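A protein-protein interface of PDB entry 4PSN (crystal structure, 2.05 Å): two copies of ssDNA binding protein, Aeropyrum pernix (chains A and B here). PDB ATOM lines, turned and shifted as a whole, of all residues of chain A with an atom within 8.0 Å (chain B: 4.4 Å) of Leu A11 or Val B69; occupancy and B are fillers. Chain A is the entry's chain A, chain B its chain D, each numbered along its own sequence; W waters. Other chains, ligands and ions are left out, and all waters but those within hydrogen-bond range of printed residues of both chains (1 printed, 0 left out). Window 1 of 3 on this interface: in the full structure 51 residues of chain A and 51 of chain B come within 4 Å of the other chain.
The indole nitrogen (NE1) of Trp A95 sits at hydrogen-bond distance from the backbone carbonyl oxygen (O) of Leu B67, at 2.8 Å. The backbone NH (N) of Val A98 lies within hydrogen-bond range of the backbone carbonyl oxygen (O) of Leu B94 (3.0 Å).
O of Val A12 lies within hydrogen-bond range of N of Val A70, at 2.9 Å. O of Asp A68 lies within hydrogen-bond range of N of Ala A14, 2.8 Å away. The side-chain carboxylate (OD2) of Asp A68 is in salt-bridge range of the guanidinium group (NH1) of Arg A96, 3.8 Å away. OD1 of Asp A68 is in hydrogen-bond range of N of Arg A97, at 3.0 Å. The backbone carbonyl oxygen (O) of Val B12 lies within hydrogen-bond range of the backbone NH (N) of Val B70 (3.0 Å). O of Val B69 is in hydrogen-bond range of N of Trp B95 (2.8 Å).
Among the printed residues, pairs that only touch across the chains: Arg A96 with Trp B95, Arg A97 with Trp B95, Trp A95 with Val B69, Trp A95 with Trp B95, Val A69 with Trp B95, Ile A103 with Leu B94, Ile A13 with Trp B95, Leu A11 with Ile B13, Ile A13 with Leu B11, Arg A97 with Leu B94, Trp A95 with Asp B68, Val A12 with Leu B11, Asp A68 with Trp B95, Leu A11 with Leu B11, Leu A11 with Val B12, Leu A11 with Val B69 and Trp A95 with Ile B13.
Of chain B, only Leu B11, Val B12, Ile B13 and Val B69 come within 4 Å of Leu A11. Arg A71 touches none of the printed residues of chain B. Of the printed residues of chain B, Trp A95 touches Ile B13 (3.98 Å), Leu B67 (2.8 Å), Asp B68 (3.8 Å), Val B69 (3.5 Å) and Trp B95 (3.5 Å). Printed residues of chain B within 4 Å of Ile A103: Leu B94. Of the printed residues of chain A, Val B12 touches Leu A11 (3.9 Å). Of the printed residues of chain A, Leu B67 touches Trp A95 (2.8 Å). Val B69 touches two residues of chain A. The nearest printed residue of chain B that does not touch Ile A13 is Glu B93 (6.0 Å).
Along chain A the printed residues that touch a printed residue of chain B span positions 11 to 103. Of the 10 printed residues of chain B, 8 touch a printed residue of chain A. Among the printed residues, no Asp or Glu carboxylate lies within 4 Å of a Lys or Arg side-chain nitrogen of the other chain.
Leu A11 touches Val B12, and with the chains exchanged Val A12 touches Leu B11. Ile A13 touches Trp B95, and with the chains exchanged Trp A95 touches Ile B13. Asp A68 touches Trp B95, and with the chains exchanged Trp A95 touches Asp B68. Trp A95 touches its own counterpart, Trp B95. 9 positions are printed for both chains. Of the 19 pairs that touch across the chains among the printed residues, 12 have their exchanged pair printed and touching as well.
Water W1 lies within hydrogen-bond range of the backbone carbonyl oxygen of Val A98 (2.8 Å) and the backbone NH of Leu B94 (2.9 Å).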
ATOM      1  N   ARG A   8       7.903  -2.809  25.212  1.00  0.00           N
ATOM      2  CA  ARG A   8       7.009  -2.379  24.129  1.00  0.00           C
ATOM      3  C   ARG A   8       5.600  -2.904  24.364  1.00  0.00           C
ATOM      4  O   ARG A   8       5.415  -4.099  24.575  1.00  0.00           O
ATOM      5  CB  ARG A   8       7.471  -2.931  22.775  1.00  0.00           C
ATOM      6  CG  ARG A   8       8.793  -2.433  22.257  1.00  0.00           C
ATOM      7  CD  ARG A   8       9.115  -3.095  20.907  1.00  0.00           C
ATOM      8  NE  ARG A   8       9.026  -4.557  20.978  1.00  0.00           N
ATOM      9  CZ  ARG A   8       8.082  -5.296  20.391  1.00  0.00           C
ATOM     10  NH1 ARG A   8       7.129  -4.719  19.668  1.00  0.00           N
ATOM     11  NH2 ARG A   8       8.095  -6.618  20.524  1.00  0.00           N
ATOM     12  N   THR A   9       4.598  -2.036  24.308  1.00  0.00           N
ATOM     13  CA  THR A   9       3.239  -2.502  24.517  1.00  0.00           C
ATOM     14  C   THR A   9       2.583  -3.014  23.242  1.00  0.00           C
ATOM     15  O   THR A   9       1.681  -3.831  23.319  1.00  0.00           O
ATOM     16  CB  THR A   9       2.320  -1.401  25.062  1.00  0.00           C
ATOM     17  OG1 THR A   9       2.258  -0.330  24.109  1.00  0.00           O
ATOM     18  CG2 THR A   9       2.835  -0.875  26.391  1.00  0.00           C
ATOM     19  N   GLY A  10       3.002  -2.516  22.081  1.00  0.00           N
ATOM     20  CA  GLY A  10       2.222  -2.729  20.874  1.00  0.00           C
ATOM     21  C   GLY A  10       0.977  -1.844  20.976  1.00  0.00           C
ATOM     22  O   GLY A  10       0.881  -1.008  21.877  1.00  0.00           O
ATOM     23  N   LEU A  11       0.029  -1.997  20.060  1.00  0.00           N
ATOM     24  CA  LEU A  11      -1.222  -1.245  20.149  1.00  0.00           C
ATOM     25  C   LEU A  11      -2.083  -1.776  21.288  1.00  0.00           C
ATOM     26  O   LEU A  11      -2.276  -2.979  21.415  1.00  0.00           O
ATOM     27  CB  LEU A  11      -2.014  -1.363  18.850  1.00  0.00           C
ATOM     28  CG  LEU A  11      -1.352  -0.869  17.566  1.00  0.00           C
ATOM     29  CD1 LEU A  11      -2.289  -1.188  16.385  1.00  0.00           C
ATOM     30  CD2 LEU A  11      -1.024   0.652  17.653  1.00  0.00           C
ATOM     31  N   VAL A  12      -2.600  -0.874  22.110  1.00  0.00           N
ATOM     32  CA  VAL A  12      -3.447  -1.274  23.221  1.00  0.00           C
ATOM     33  C   VAL A  12      -4.499  -0.197  23.524  1.00  0.00           C
ATOM     34  O   VAL A  12      -4.244   0.990  23.384  1.00  0.00           O
ATOM     35  CB  VAL A  12      -2.587  -1.636  24.475  1.00  0.00           C
ATOM     36  CG1 VAL A  12      -1.895  -0.398  25.052  1.00  0.00           C
ATOM     37  CG2 VAL A  12      -3.423  -2.340  25.526  1.00  0.00           C
ATOM     38  N   ILE A  13      -5.704  -0.621  23.886  1.00  0.00           N
ATOM     39  CA  ILE A  13      -6.743   0.315  24.313  1.00  0.00           C
ATOM     40  C   ILE A  13      -6.236   0.975  25.590  1.00  0.00           C
ATOM     41  O   ILE A  13      -5.636   0.312  26.444  1.00  0.00           O
ATOM     42  CB  ILE A  13      -8.094  -0.393  24.563  1.00  0.00           C
ATOM     43  CG1 ILE A  13      -8.686  -0.884  23.243  1.00  0.00           C
ATOM     44  CG2 ILE A  13      -9.092   0.560  25.175  1.00  0.00           C
ATOM     45  CD1 ILE A  13      -9.163   0.271  22.355  1.00  0.00           C
ATOM     46  N   ALA A  14      -6.421   2.281  25.707  1.00  0.00           N
ATOM     47  CA  ALA A  14      -5.767   3.036  26.782  1.00  0.00           C
ATOM     48  C   ALA A  14      -6.118   2.527  28.178  1.00  0.00           C
ATOM     49  O   ALA A  14      -5.255   2.488  29.059  1.00  0.00           O
ATOM     50  CB  ALA A  14      -6.042   4.543  26.652  1.00  0.00           C
ATOM     51  N   LYS A  20      -0.902  -4.331  30.268  1.00  0.00           N
ATOM     52  CA  LYS A  20       0.000  -4.733  29.181  1.00  0.00           C
ATOM     53  C   LYS A  20       1.463  -4.478  29.568  1.00  0.00           C
ATOM     54  O   LYS A  20       2.343  -5.321  29.350  1.00  0.00           O
ATOM     55  CB  LYS A  20      -0.348  -4.026  27.865  1.00  0.00           C
ATOM     56  CG  LYS A  20       0.559  -4.435  26.702  1.00  0.00           C
ATOM     57  CD  LYS A  20       0.297  -5.857  26.255  1.00  0.00           C
ATOM     58  CE  LYS A  20      -0.989  -5.950  25.439  1.00  0.00           C
ATOM     59  NZ  LYS A  20      -0.887  -6.993  24.369  1.00  0.00           N
ATOM     60  N   ASP A  68      -9.379   5.346  23.823  1.00  0.00           N
ATOM     61  CA  ASP A  68      -8.411   5.640  22.779  1.00  0.00           C
ATOM     62  C   ASP A  68      -7.396   4.486  22.653  1.00  0.00           C
ATOM     63  O   ASP A  68      -7.433   3.517  23.424  1.00  0.00           O
ATOM     64  CB  ASP A  68      -7.690   6.967  23.057  1.00  0.00           C
ATOM     65  CG  ASP A  68      -8.601   8.198  22.891  1.00  0.00           C
ATOM     66  OD1 ASP A  68      -9.621   8.122  22.178  1.00  0.00           O
ATOM     67  OD2 ASP A  68      -8.280   9.260  23.468  1.00  0.00           O
ATOM     68  N   VAL A  69      -6.499   4.597  21.674  1.00  0.00           N
ATOM     69  CA  VAL A  69      -5.439   3.619  21.474  1.00  0.00           C
ATOM     70  C   VAL A  69      -4.092   4.270  21.738  1.00  0.00           C
ATOM     71  O   VAL A  69      -3.870   5.426  21.358  1.00  0.00           O
ATOM     72  CB  VAL A  69      -5.463   3.022  20.051  1.00  0.00           C
ATOM     73  CG1 VAL A  69      -4.213   2.145  19.809  1.00  0.00           C
ATOM     74  CG2 VAL A  69      -6.745   2.193  19.843  1.00  0.00           C
ATOM     75  N   VAL A  70      -3.206   3.548  22.419  1.00  0.00           N
ATOM     76  CA  VAL A  70      -1.864   4.067  22.668  1.00  0.00           C
ATOM     77  C   VAL A  70      -0.862   2.979  22.346  1.00  0.00           C
ATOM     78  O   VAL A  70      -1.214   1.804  22.226  1.00  0.00           O
ATOM     79  CB  VAL A  70      -1.655   4.555  24.135  1.00  0.00           C
ATOM     80  CG1 VAL A  70      -2.656   5.632  24.490  1.00  0.00           C
ATOM     81  CG2 VAL A  70      -1.776   3.397  25.113  1.00  0.00           C
ATOM     82  N   ARG A  71       0.380   3.388  22.154  1.00  0.00           N
ATOM     83  CA  ARG A  71       1.472   2.452  21.995  1.00  0.00           C
ATOM     84  C   ARG A  71       2.666   3.097  22.646  1.00  0.00           C
ATOM     85  O   ARG A  71       2.957   4.275  22.412  1.00  0.00           O
ATOM     86  CB  ARG A  71       1.759   2.144  20.524  1.00  0.00           C
ATOM     87  CG  ARG A  71       2.938   1.215  20.333  1.00  0.00           C
ATOM     88  CD  ARG A  71       2.934   0.578  18.939  1.00  0.00           C
ATOM     89  NE  ARG A  71       3.123   1.542  17.862  1.00  0.00           N
ATOM     90  CZ  ARG A  71       2.986   1.252  16.566  1.00  0.00           C
ATOM     91  NH1 ARG A  71       3.184   2.188  15.651  1.00  0.00           N
ATOM     92  NH2 ARG A  71       2.632   0.024  16.187  1.00  0.00           N
ATOM     93  N   ILE A  72       3.345   2.328  23.485  1.00  0.00           N
ATOM     94  CA  ILE A  72       4.367   2.883  24.352  1.00  0.00           C
ATOM     95  C   ILE A  72       5.629   2.077  24.292  1.00  0.00           C
ATOM     96  O   ILE A  72       5.589   0.851  24.266  1.00  0.00           O
ATOM     97  CB  ILE A  72       3.887   2.873  25.813  1.00  0.00           C
ATOM     98  CG1 ILE A  72       2.620   3.718  25.956  1.00  0.00           C
ATOM     99  CG2 ILE A  72       4.973   3.392  26.727  1.00  0.00           C
ATOM    100  CD1 ILE A  72       1.869   3.476  27.233  1.00  0.00           C
ATOM    101  N   GLU A  93       2.709   6.910  21.413  1.00  0.00           N
ATOM    102  CA  GLU A  93       1.883   7.257  20.265  1.00  0.00           C
ATOM    103  C   GLU A  93       0.445   7.237  20.734  1.00  0.00           C
ATOM    104  O   GLU A  93       0.081   6.439  21.598  1.00  0.00           O
ATOM    105  CB  GLU A  93       2.083   6.266  19.115  1.00  0.00           C
ATOM    106  CG  GLU A  93       3.429   6.372  18.400  1.00  0.00           C
ATOM    107  CD  GLU A  93       3.807   5.069  17.726  1.00  0.00           C
ATOM    108  OE1 GLU A  93       4.193   4.116  18.446  1.00  0.00           O
ATOM    109  OE2 GLU A  93       3.699   4.989  16.484  1.00  0.00           O
ATOM    110  N   LEU A  94      -0.376   8.119  20.179  1.00  0.00           N
ATOM    111  CA  LEU A  94      -1.765   8.201  20.586  1.00  0.00           C
ATOM    112  C   LEU A  94      -2.657   8.288  19.351  1.00  0.00           C
ATOM    113  O   LEU A  94      -2.324   8.984  18.385  1.00  0.00           O
ATOM    114  CB  LEU A  94      -1.981   9.426  21.485  1.00  0.00           C
ATOM    115  CG  LEU A  94      -3.427   9.774  21.858  1.00  0.00           C
ATOM    116  CD1 LEU A  94      -4.096   8.635  22.615  1.00  0.00           C
ATOM    117  CD2 LEU A  94      -3.483  11.064  22.682  1.00  0.00           C
ATOM    118  N   TRP A  95      -3.771   7.559  19.385  1.00  0.00           N
ATOM    119  CA  TRP A  95      -4.771   7.609  18.323  1.00  0.00           C
ATOM    120  C   TRP A  95      -6.099   7.871  19.003  1.00  0.00           C
ATOM    121  O   TRP A  95      -6.462   7.161  19.946  1.00  0.00           O
ATOM    122  CB  TRP A  95      -4.869   6.271  17.579  1.00  0.00           C
ATOM    123  CG  TRP A  95      -3.660   5.865  16.745  1.00  0.00           C
ATOM    124  CD1 TRP A  95      -3.528   5.972  15.382  1.00  0.00           C
ATOM    125  CD2 TRP A  95      -2.436   5.245  17.211  1.00  0.00           C
ATOM    126  NE1 TRP A  95      -2.304   5.476  14.982  1.00  0.00           N
ATOM    127  CE2 TRP A  95      -1.621   5.028  16.076  1.00  0.00           C
ATOM    128  CE3 TRP A  95      -1.959   4.873  18.473  1.00  0.00           C
ATOM    129  CZ2 TRP A  95      -0.346   4.446  16.169  1.00  0.00           C
ATOM    130  CZ3 TRP A  95      -0.682   4.277  18.555  1.00  0.00           C
ATOM    131  CH2 TRP A  95       0.095   4.073  17.415  1.00  0.00           C
ATOM    132  N   ARG A  96      -6.829   8.875  18.526  1.00  0.00           N
ATOM    133  CA  ARG A  96      -8.091   9.240  19.152  1.00  0.00           C
ATOM    134  C   ARG A  96      -9.289   8.599  18.455  1.00  0.00           C
ATOM    135  O   ARG A  96      -9.401   8.610  17.221  1.00  0.00           O
ATOM    136  CB  ARG A  96      -8.241  10.770  19.224  1.00  0.00           C
ATOM    137  CG  ARG A  96      -7.129  11.449  20.018  1.00  0.00           C
ATOM    138  CD  ARG A  96      -7.541  12.829  20.478  1.00  0.00           C
ATOM    139  NE  ARG A  96      -6.450  13.539  21.144  1.00  0.00           N
ATOM    140  CZ  ARG A  96      -6.210  13.503  22.453  1.00  0.00           C
ATOM    141  NH1 ARG A  96      -6.976  12.781  23.265  1.00  0.00           N
ATOM    142  NH2 ARG A  96      -5.191  14.193  22.949  1.00  0.00           N
ATOM    143  N   ARG A  97     -10.168   8.027  19.269  1.00  0.00           N
ATOM    144  CA  ARG A  97     -11.345   7.311  18.802  1.00  0.00           C
ATOM    145  C   ARG A  97     -12.286   8.212  17.992  1.00  0.00           C
ATOM    146  O   ARG A  97     -12.618   9.310  18.413  1.00  0.00           O
ATOM    147  CB  ARG A  97     -12.095   6.748  20.016  1.00  0.00           C
ATOM    148  CG  ARG A  97     -13.167   5.704  19.715  1.00  0.00           C
ATOM    149  CD  ARG A  97     -13.895   5.307  21.007  1.00  0.00           C
ATOM    150  NE  ARG A  97     -14.507   6.474  21.642  1.00  0.00           N
ATOM    151  CZ  ARG A  97     -15.802   6.775  21.563  1.00  0.00           C
ATOM    152  NH1 ARG A  97     -16.270   7.870  22.155  1.00  0.00           N
ATOM    153  NH2 ARG A  97     -16.634   5.979  20.892  1.00  0.00           N
ATOM    154  N   VAL A  98     -12.703   7.740  16.826  1.00  0.00           N
ATOM    155  CA  VAL A  98     -13.777   8.378  16.076  1.00  0.00           C
ATOM    156  C   VAL A  98     -15.106   7.939  16.688  1.00  0.00           C
ATOM    157  O   VAL A  98     -15.342   6.743  16.862  1.00  0.00           O
ATOM    158  CB  VAL A  98     -13.744   7.959  14.601  1.00  0.00           C
ATOM    159  CG1 VAL A  98     -14.940   8.533  13.855  1.00  0.00           C
ATOM    160  CG2 VAL A  98     -12.440   8.418  13.956  1.00  0.00           C
ATOM    161  N   ILE A 103     -19.196   7.130  12.444  1.00  0.00           N
ATOM    162  CA  ILE A 103     -18.846   5.909  11.720  1.00  0.00           C
ATOM    163  C   ILE A 103     -20.042   5.040  11.380  1.00  0.00           C
ATOM    164  O   ILE A 103     -20.136   4.535  10.269  1.00  0.00           O
ATOM    165  CB  ILE A 103     -17.842   5.039  12.500  1.00  0.00           C
ATOM    166  CG1 ILE A 103     -16.492   5.731  12.602  1.00  0.00           C
ATOM    167  CG2 ILE A 103     -17.640   3.695  11.812  1.00  0.00           C
ATOM    168  CD1 ILE A 103     -15.413   4.816  13.127  1.00  0.00           C
ATOM    169  N   LEU B  11      -6.955  -4.803  17.157  1.00  0.00           N
ATOM    170  CA  LEU B  11      -6.385  -3.519  16.747  1.00  0.00           C
ATOM    171  C   LEU B  11      -5.296  -3.769  15.723  1.00  0.00           C
ATOM    172  O   LEU B  11      -4.444  -4.621  15.928  1.00  0.00           O
ATOM    173  CB  LEU B  11      -5.770  -2.796  17.946  1.00  0.00           C
ATOM    174  CG  LEU B  11      -6.671  -2.526  19.158  1.00  0.00           C
ATOM    175  CD1 LEU B  11      -5.856  -1.895  20.298  1.00  0.00           C
ATOM    176  CD2 LEU B  11      -7.839  -1.616  18.752  1.00  0.00           C
ATOM    177  N   VAL B  12      -5.307  -3.011  14.631  1.00  0.00           N
ATOM    178  CA  VAL B  12      -4.275  -3.147  13.609  1.00  0.00           C
ATOM    179  C   VAL B  12      -4.024  -1.793  12.942  1.00  0.00           C
ATOM    180  O   VAL B  12      -4.949  -1.012  12.741  1.00  0.00           O
ATOM    181  CB  VAL B  12      -4.671  -4.210  12.541  1.00  0.00           C
ATOM    182  CG1 VAL B  12      -5.951  -3.804  11.825  1.00  0.00           C
ATOM    183  CG2 VAL B  12      -3.536  -4.430  11.518  1.00  0.00           C
ATOM    184  N   ILE B  13      -2.771  -1.498  12.627  1.00  0.00           N
ATOM    185  CA  ILE B  13      -2.488  -0.301  11.847  1.00  0.00           C
ATOM    186  C   ILE B  13      -3.256  -0.439  10.521  1.00  0.00           C
ATOM    187  O   ILE B  13      -3.299  -1.532   9.945  1.00  0.00           O
ATOM    188  CB  ILE B  13      -0.962  -0.133  11.595  1.00  0.00           C
ATOM    189  CG1 ILE B  13      -0.235   0.085  12.923  1.00  0.00           C
ATOM    190  CG2 ILE B  13      -0.688   1.054  10.692  1.00  0.00           C
ATOM    191  CD1 ILE B  13      -0.564   1.420  13.588  1.00  0.00           C
ATOM    192  N   LEU B  67      -1.542   5.226   8.661  1.00  0.00           N
ATOM    193  CA  LEU B  67      -1.012   5.084  10.013  1.00  0.00           C
ATOM    194  C   LEU B  67      -2.069   5.260  11.100  1.00  0.00           C
ATOM    195  O   LEU B  67      -1.738   5.421  12.269  1.00  0.00           O
ATOM    196  CB  LEU B  67       0.169   6.030  10.242  1.00  0.00           C
ATOM    197  CG  LEU B  67       1.428   5.613   9.473  1.00  0.00           C
ATOM    198  CD1 LEU B  67       2.608   6.506   9.835  1.00  0.00           C
ATOM    199  CD2 LEU B  67       1.768   4.138   9.725  1.00  0.00           C
ATOM    200  N   ASP B  68      -3.342   5.228  10.719  1.00  0.00           N
ATOM    201  CA  ASP B  68      -4.396   5.223  11.719  1.00  0.00           C
ATOM    202  C   ASP B  68      -4.561   3.801  12.285  1.00  0.00           C
ATOM    203  O   ASP B  68      -3.880   2.872  11.862  1.00  0.00           O
ATOM    204  CB  ASP B  68      -5.711   5.729  11.119  1.00  0.00           C
ATOM    205  CG  ASP B  68      -5.724   7.233  10.914  1.00  0.00           C
ATOM    206  OD1 ASP B  68      -4.970   7.954  11.620  1.00  0.00           O
ATOM    207  OD2 ASP B  68      -6.507   7.695  10.053  1.00  0.00           O
ATOM    208  N   VAL B  69      -5.442   3.635  13.255  1.00  0.00           N
ATOM    209  CA  VAL B  69      -5.686   2.299  13.805  1.00  0.00           C
ATOM    210  C   VAL B  69      -7.136   1.915  13.510  1.00  0.00           C
ATOM    211  O   VAL B  69      -8.020   2.755  13.596  1.00  0.00           O
ATOM    212  CB  VAL B  69      -5.410   2.245  15.331  1.00  0.00           C
ATOM    213  CG1 VAL B  69      -5.860   0.891  15.922  1.00  0.00           C
ATOM    214  CG2 VAL B  69      -3.917   2.475  15.617  1.00  0.00           C
ATOM    215  N   VAL B  70      -7.372   0.664  13.128  1.00  0.00           N
ATOM    216  CA  VAL B  70      -8.739   0.179  12.926  1.00  0.00           C
ATOM    217  C   VAL B  70      -8.958  -1.152  13.645  1.00  0.00           C
ATOM    218  O   VAL B  70      -8.015  -1.862  14.001  1.00  0.00           O
ATOM    219  CB  VAL B  70      -9.083  -0.020  11.421  1.00  0.00           C
ATOM    220  CG1 VAL B  70      -8.931   1.281  10.626  1.00  0.00           C
ATOM    221  CG2 VAL B  70      -8.219  -1.119  10.826  1.00  0.00           C
ATOM    222  N   GLU B  93     -14.255   0.007  13.766  1.00  0.00           N
ATOM    223  CA  GLU B  93     -13.850   1.094  14.663  1.00  0.00           C
ATOM    224  C   GLU B  93     -12.625   1.760  14.070  1.00  0.00           C
ATOM    225  O   GLU B  93     -11.822   1.097  13.423  1.00  0.00           O
ATOM    226  CB  GLU B  93     -13.523   0.575  16.055  1.00  0.00           C
ATOM    227  CG  GLU B  93     -14.722   0.068  16.847  1.00  0.00           C
ATOM    228  CD  GLU B  93     -14.292  -0.894  17.930  1.00  0.00           C
ATOM    229  OE1 GLU B  93     -14.099  -2.086  17.613  1.00  0.00           O
ATOM    230  OE2 GLU B  93     -14.111  -0.461  19.088  1.00  0.00           O
ATOM    231  N   LEU B  94     -12.506   3.069  14.258  1.00  0.00           N
ATOM    232  CA  LEU B  94     -11.391   3.829  13.696  1.00  0.00           C
ATOM    233  C   LEU B  94     -10.791   4.731  14.759  1.00  0.00           C
ATOM    234  O   LEU B  94     -11.511   5.376  15.497  1.00  0.00           O
ATOM    235  CB  LEU B  94     -11.874   4.685  12.518  1.00  0.00           C
ATOM    236  CG  LEU B  94     -10.847   5.584  11.821  1.00  0.00           C
ATOM    237  CD1 LEU B  94      -9.645   4.783  11.311  1.00  0.00           C
ATOM    238  CD2 LEU B  94     -11.492   6.376  10.674  1.00  0.00           C
ATOM    239  N   TRP B  95      -9.469   4.771  14.844  1.00  0.00           N
ATOM    240  CA  TRP B  95      -8.820   5.764  15.693  1.00  0.00           C
ATOM    241  C   TRP B  95      -7.861   6.566  14.819  1.00  0.00           C
ATOM    242  O   TRP B  95      -7.101   5.987  14.033  1.00  0.00           O
ATOM    243  CB  TRP B  95      -8.043   5.091  16.824  1.00  0.00           C
ATOM    244  CG  TRP B  95      -8.860   4.335  17.828  1.00  0.00           C
ATOM    245  CD1 TRP B  95      -9.228   4.765  19.072  1.00  0.00           C
ATOM    246  CD2 TRP B  95      -9.374   3.009  17.689  1.00  0.00           C
ATOM    247  NE1 TRP B  95      -9.958   3.793  19.714  1.00  0.00           N
ATOM    248  CE2 TRP B  95     -10.060   2.699  18.891  1.00  0.00           C
ATOM    249  CE3 TRP B  95      -9.344   2.051  16.664  1.00  0.00           C
ATOM    250  CZ2 TRP B  95     -10.690   1.469  19.104  1.00  0.00           C
ATOM    251  CZ3 TRP B  95      -9.972   0.818  16.877  1.00  0.00           C
ATOM    252  CH2 TRP B  95     -10.635   0.542  18.090  1.00  0.00           C
HETATM  253  O   HOH W   1     -14.543   4.212  16.046  1.00  0.00           O
